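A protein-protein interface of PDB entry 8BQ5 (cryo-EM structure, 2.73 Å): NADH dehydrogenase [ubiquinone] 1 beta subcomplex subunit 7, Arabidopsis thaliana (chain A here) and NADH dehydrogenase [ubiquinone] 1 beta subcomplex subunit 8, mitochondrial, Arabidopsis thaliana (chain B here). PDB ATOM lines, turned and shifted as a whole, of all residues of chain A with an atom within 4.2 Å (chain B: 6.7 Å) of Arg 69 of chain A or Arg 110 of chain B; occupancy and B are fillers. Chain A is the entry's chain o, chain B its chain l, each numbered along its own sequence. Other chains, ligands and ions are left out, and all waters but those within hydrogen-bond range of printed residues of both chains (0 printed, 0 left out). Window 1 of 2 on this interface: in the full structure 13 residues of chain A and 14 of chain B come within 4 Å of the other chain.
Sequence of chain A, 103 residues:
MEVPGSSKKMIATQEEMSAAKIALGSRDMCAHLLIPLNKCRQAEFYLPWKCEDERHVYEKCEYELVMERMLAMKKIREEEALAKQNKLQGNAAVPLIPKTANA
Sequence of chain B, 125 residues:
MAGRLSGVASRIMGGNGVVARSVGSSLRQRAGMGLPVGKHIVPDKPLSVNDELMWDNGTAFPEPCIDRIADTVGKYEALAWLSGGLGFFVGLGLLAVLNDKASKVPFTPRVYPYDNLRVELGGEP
Arg 110 of chain B touches just one residue of chain A: Arg 69 (3.5 Å). Printed residues of chain A within 4 Å of Phe 107 of chain B: Arg 69 and Met 73. Of the printed residues of chain A, Thr 108 of chain B touches Arg 69 (2.6 Å), Ala 72 (3.8 Å) and Met 73 (3.5 Å). Val 111 of chain B touches none of the printed residues of chain A. The nearest printed residue of chain A that does not touch Arg 110 of chain B is Val 66 of chain A (6.2 Å). The nearest printed residue of chain B that does not touch Met 70 of chain A is Phe 107 of chain B (4.02 Å).
The backbone carbonyl oxygen of Thr 108 of chain B sits at hydrogen-bond distance from the guanidinium group of Arg 69 of chain A.
NH1 of Arg 110 of chain B lies within hydrogen-bond range of OH of Tyr 112 of chain B (3.3 Å).
Along chain A the printed residues that touch a printed residue of chain B span positions 69 to 73. Hydrophobic or aromatic side chains of chain B that line the printed part of chain A: Phe 107. Among the printed residues, no Asp or Glu carboxylate lies within 4 Å of a Lys or Arg side-chain nitrogen of the other chain.
Arg 69 of chain A touches Phe 107 of chain B. NE of Arg 69 of chain A touches C of Pro 109 of chain B (3.8 Å). NH1 of Arg 69 of chain A touches CG of Arg 110 of chain B, at 3.5 Å. CG of Met 70 of chain A touches O of Pro 106 of chain B, at 3.6 Å. Ala 72 of chain A touches Thr 108 of chain B (CB to CG2, 3.8 Å). Met 73 of chain A touches Pro 106 of chain B. Met 73 of chain A touches Phe 107 of chain B. CE of Met 73 of chain A touches CG2 of Thr 108 of chain B, 3.5 Å away.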
ATOM      1  N   LEU A  65      14.948   3.745   6.260  1.00  0.00           N
ATOM      2  CA  LEU A  65      14.413   4.967   6.847  1.00  0.00           C
ATOM      3  C   LEU A  65      13.442   4.635   7.973  1.00  0.00           C
ATOM      4  O   LEU A  65      13.424   5.292   9.017  1.00  0.00           O
ATOM      5  CB  LEU A  65      13.726   5.799   5.766  1.00  0.00           C
ATOM      6  CG  LEU A  65      14.597   6.739   4.930  1.00  0.00           C
ATOM      7  CD1 LEU A  65      13.748   7.466   3.904  1.00  0.00           C
ATOM      8  CD2 LEU A  65      15.339   7.727   5.809  1.00  0.00           C
ATOM      9  N   VAL A  66      12.614   3.615   7.774  1.00  0.00           N
ATOM     10  CA  VAL A  66      11.679   3.207   8.818  1.00  0.00           C
ATOM     11  C   VAL A  66      12.426   2.635  10.018  1.00  0.00           C
ATOM     12  O   VAL A  66      12.096   2.935  11.174  1.00  0.00           O
ATOM     13  CB  VAL A  66      10.658   2.209   8.242  1.00  0.00           C
ATOM     14  CG1 VAL A  66      10.169   1.248   9.312  1.00  0.00           C
ATOM     15  CG2 VAL A  66       9.489   2.955   7.621  1.00  0.00           C
ATOM     16  N   MET A  67      13.442   1.805   9.766  1.00  0.00           N
ATOM     17  CA  MET A  67      14.205   1.214  10.862  1.00  0.00           C
ATOM     18  C   MET A  67      14.913   2.285  11.680  1.00  0.00           C
ATOM     19  O   MET A  67      14.912   2.234  12.916  1.00  0.00           O
ATOM     20  CB  MET A  67      15.216   0.206  10.318  1.00  0.00           C
ATOM     21  CG  MET A  67      14.597  -1.028   9.689  1.00  0.00           C
ATOM     22  SD  MET A  67      13.569  -1.970  10.829  1.00  0.00           S
ATOM     23  CE  MET A  67      11.977  -1.817  10.028  1.00  0.00           C
ATOM     24  N   GLU A  68      15.515   3.271  11.005  1.00  0.00           N
ATOM     25  CA  GLU A  68      16.132   4.388  11.715  1.00  0.00           C
ATOM     26  C   GLU A  68      15.127   5.090  12.620  1.00  0.00           C
ATOM     27  O   GLU A  68      15.423   5.369  13.788  1.00  0.00           O
ATOM     28  CB  GLU A  68      16.759   5.383  10.726  1.00  0.00           C
ATOM     29  CG  GLU A  68      17.482   6.534  11.382  1.00  0.00           C
ATOM     30  CD  GLU A  68      18.124   7.464  10.406  1.00  0.00           C
ATOM     31  OE1 GLU A  68      17.990   7.254   9.180  1.00  0.00           O
ATOM     32  OE2 GLU A  68      18.775   8.415  10.858  1.00  0.00           O
ATOM     33  N   ARG A  69      13.926   5.370  12.107  1.00  0.00           N
ATOM     34  CA  ARG A  69      12.911   6.023  12.919  1.00  0.00           C
ATOM     35  C   ARG A  69      12.360   5.075  13.968  1.00  0.00           C
ATOM     36  O   ARG A  69      11.824   5.524  14.985  1.00  0.00           O
ATOM     37  CB  ARG A  69      11.790   6.560  12.029  1.00  0.00           C
ATOM     38  CG  ARG A  69      12.092   7.900  11.391  1.00  0.00           C
ATOM     39  CD  ARG A  69      11.043   8.246  10.361  1.00  0.00           C
ATOM     40  NE  ARG A  69       9.704   8.011  10.880  1.00  0.00           N
ATOM     41  CZ  ARG A  69       8.757   7.352  10.228  1.00  0.00           C
ATOM     42  NH1 ARG A  69       8.969   6.854   9.021  1.00  0.00           N
ATOM     43  NH2 ARG A  69       7.571   7.185  10.802  1.00  0.00           N
ATOM     44  N   MET A  70      12.476   3.767  13.739  1.00  0.00           N
ATOM     45  CA  MET A  70      12.152   2.812  14.791  1.00  0.00           C
ATOM     46  C   MET A  70      13.228   2.806  15.868  1.00  0.00           C
ATOM     47  O   MET A  70      12.917   2.762  17.064  1.00  0.00           O
ATOM     48  CB  MET A  70      11.976   1.416  14.200  1.00  0.00           C
ATOM     49  CG  MET A  70      10.589   1.139  13.658  1.00  0.00           C
ATOM     50  SD  MET A  70      10.511  -0.459  12.838  1.00  0.00           S
ATOM     51  CE  MET A  70       9.559  -1.405  14.020  1.00  0.00           C
ATOM     52  N   LEU A  71      14.500   2.851  15.462  1.00  0.00           N
ATOM     53  CA  LEU A  71      15.583   2.941  16.435  1.00  0.00           C
ATOM     54  C   LEU A  71      15.509   4.243  17.221  1.00  0.00           C
ATOM     55  O   LEU A  71      15.767   4.260  18.429  1.00  0.00           O
ATOM     56  CB  LEU A  71      16.938   2.814  15.736  1.00  0.00           C
ATOM     57  CG  LEU A  71      17.282   1.484  15.052  1.00  0.00           C
ATOM     58  CD1 LEU A  71      18.595   1.570  14.283  1.00  0.00           C
ATOM     59  CD2 LEU A  71      17.298   0.321  16.039  1.00  0.00           C
ATOM     60  N   ALA A  72      15.156   5.342  16.550  1.00  0.00           N
ATOM     61  CA  ALA A  72      15.045   6.624  17.235  1.00  0.00           C
ATOM     62  C   ALA A  72      13.988   6.570  18.330  1.00  0.00           C
ATOM     63  O   ALA A  72      14.201   7.067  19.441  1.00  0.00           O
ATOM     64  CB  ALA A  72      14.727   7.729  16.228  1.00  0.00           C
ATOM     65  N   MET A  73      12.839   5.956  18.037  1.00  0.00           N
ATOM     66  CA  MET A  73      11.781   5.863  19.037  1.00  0.00           C
ATOM     67  C   MET A  73      12.158   4.924  20.175  1.00  0.00           C
ATOM     68  O   MET A  73      11.742   5.145  21.318  1.00  0.00           O
ATOM     69  CB  MET A  73      10.472   5.420  18.377  1.00  0.00           C
ATOM     70  CG  MET A  73       9.301   5.192  19.337  1.00  0.00           C
ATOM     71  SD  MET A  73       8.666   6.571  20.332  1.00  0.00           S
ATOM     72  CE  MET A  73       9.248   8.041  19.487  1.00  0.00           C
ATOM     73  N   PRO B 106       5.561   2.668  17.591  1.00  0.00           N
ATOM     74  CA  PRO B 106       6.949   2.209  17.637  1.00  0.00           C
ATOM     75  C   PRO B 106       7.925   2.934  16.703  1.00  0.00           C
ATOM     76  O   PRO B 106       9.034   2.457  16.570  1.00  0.00           O
ATOM     77  CB  PRO B 106       6.847   0.729  17.211  1.00  0.00           C
ATOM     78  CG  PRO B 106       5.393   0.508  16.822  1.00  0.00           C
ATOM     79  CD  PRO B 106       4.784   1.881  16.645  1.00  0.00           C
ATOM     80  N   PHE B 107       7.516   4.054  16.106  1.00  0.00           N
ATOM     81  CA  PHE B 107       8.409   4.840  15.271  1.00  0.00           C
ATOM     82  C   PHE B 107       8.100   6.319  15.443  1.00  0.00           C
ATOM     83  O   PHE B 107       6.972   6.701  15.762  1.00  0.00           O
ATOM     84  CB  PHE B 107       8.289   4.429  13.794  1.00  0.00           C
ATOM     85  CG  PHE B 107       6.870   4.279  13.317  1.00  0.00           C
ATOM     86  CD1 PHE B 107       6.112   5.390  12.986  1.00  0.00           C
ATOM     87  CD2 PHE B 107       6.292   3.024  13.205  1.00  0.00           C
ATOM     88  CE1 PHE B 107       4.809   5.256  12.548  1.00  0.00           C
ATOM     89  CE2 PHE B 107       4.987   2.883  12.769  1.00  0.00           C
ATOM     90  CZ  PHE B 107       4.245   4.001  12.442  1.00  0.00           C
ATOM     91  N   THR B 108       9.119   7.148  15.228  1.00  0.00           N
ATOM     92  CA  THR B 108       8.954   8.587  15.303  1.00  0.00           C
ATOM     93  C   THR B 108       8.180   9.094  14.089  1.00  0.00           C
ATOM     94  O   THR B 108       8.125   8.427  13.054  1.00  0.00           O
ATOM     95  CB  THR B 108      10.314   9.276  15.372  1.00  0.00           C
ATOM     96  OG1 THR B 108      11.043   9.009  14.169  1.00  0.00           O
ATOM     97  CG2 THR B 108      11.110   8.772  16.557  1.00  0.00           C
ATOM     98  N   PRO B 109       7.561  10.269  14.193  1.00  0.00           N
ATOM     99  CA  PRO B 109       6.923  10.860  13.013  1.00  0.00           C
ATOM    100  C   PRO B 109       7.942  11.184  11.933  1.00  0.00           C
ATOM    101  O   PRO B 109       9.092  11.531  12.213  1.00  0.00           O
ATOM    102  CB  PRO B 109       6.265  12.135  13.557  1.00  0.00           C
ATOM    103  CG  PRO B 109       6.190  11.945  15.031  1.00  0.00           C
ATOM    104  CD  PRO B 109       7.348  11.080  15.404  1.00  0.00           C
ATOM    105  N   ARG B 110       7.502  11.059  10.683  1.00  0.00           N
ATOM    106  CA  ARG B 110       8.351  11.391   9.550  1.00  0.00           C
ATOM    107  C   ARG B 110       8.767  12.856   9.607  1.00  0.00           C
ATOM    108  O   ARG B 110       7.996  13.730  10.013  1.00  0.00           O
ATOM    109  CB  ARG B 110       7.624  11.122   8.230  1.00  0.00           C
ATOM    110  CG  ARG B 110       7.211   9.679   7.976  1.00  0.00           C
ATOM    111  CD  ARG B 110       6.660   9.542   6.561  1.00  0.00           C
ATOM    112  NE  ARG B 110       5.876   8.326   6.365  1.00  0.00           N
ATOM    113  CZ  ARG B 110       5.842   7.633   5.235  1.00  0.00           C
ATOM    114  NH1 ARG B 110       6.528   8.012   4.170  1.00  0.00           N
ATOM    115  NH2 ARG B 110       5.094   6.534   5.171  1.00  0.00           N
ATOM    116  N   VAL B 111      10.007  13.121   9.205  1.00  0.00           N
ATOM    117  CA  VAL B 111      10.509  14.482   9.058  1.00  0.00           C
ATOM    118  C   VAL B 111      10.980  14.619   7.618  1.00  0.00           C
ATOM    119  O   VAL B 111      11.885  13.894   7.187  1.00  0.00           O
ATOM    120  CB  VAL B 111      11.647  14.807  10.036  1.00  0.00           C
ATOM    121  CG1 VAL B 111      12.348  16.092   9.625  1.00  0.00           C
ATOM    122  CG2 VAL B 111      11.112  14.917  11.452  1.00  0.00           C
ATOM    123  N   TYR B 112      10.376  15.537   6.875  1.00  0.00           N
ATOM    124  CA  TYR B 112      10.665  15.673   5.460  1.00  0.00           C
ATOM    125  C   TYR B 112      11.697  16.771   5.215  1.00  0.00           C
ATOM    126  O   TYR B 112      11.783  17.740   5.971  1.00  0.00           O
ATOM    127  CB  TYR B 112       9.376  15.961   4.695  1.00  0.00           C
ATOM    128  CG  TYR B 112       8.547  14.720   4.446  1.00  0.00           C
ATOM    129  CD1 TYR B 112       7.760  14.170   5.450  1.00  0.00           C
ATOM    130  CD2 TYR B 112       8.558  14.094   3.207  1.00  0.00           C
ATOM    131  CE1 TYR B 112       7.007  13.031   5.225  1.00  0.00           C
ATOM    132  CE2 TYR B 112       7.808  12.959   2.972  1.00  0.00           C
ATOM    133  CZ  TYR B 112       7.035  12.432   3.983  1.00  0.00           C
ATOM    134  OH  TYR B 112       6.291  11.301   3.747  1.00  0.00           O
ATOM    135  N   ASN B 116      10.342  20.493   5.962  1.00  0.00           N
ATOM    136  CA  ASN B 116       9.167  19.621   5.918  1.00  0.00           C
ATOM    137  C   ASN B 116       8.259  19.970   4.741  1.00  0.00           C
ATOM    138  O   ASN B 116       7.035  20.016   4.872  1.00  0.00           O
ATOM    139  CB  ASN B 116       8.390  19.670   7.235  1.00  0.00           C
ATOM    140  CG  ASN B 116       7.349  18.579   7.333  1.00  0.00           C
ATOM    141  OD1 ASN B 116       7.522  17.490   6.782  1.00  0.00           O
ATOM    142  ND2 ASN B 116       6.263  18.859   8.042  1.00  0.00           N
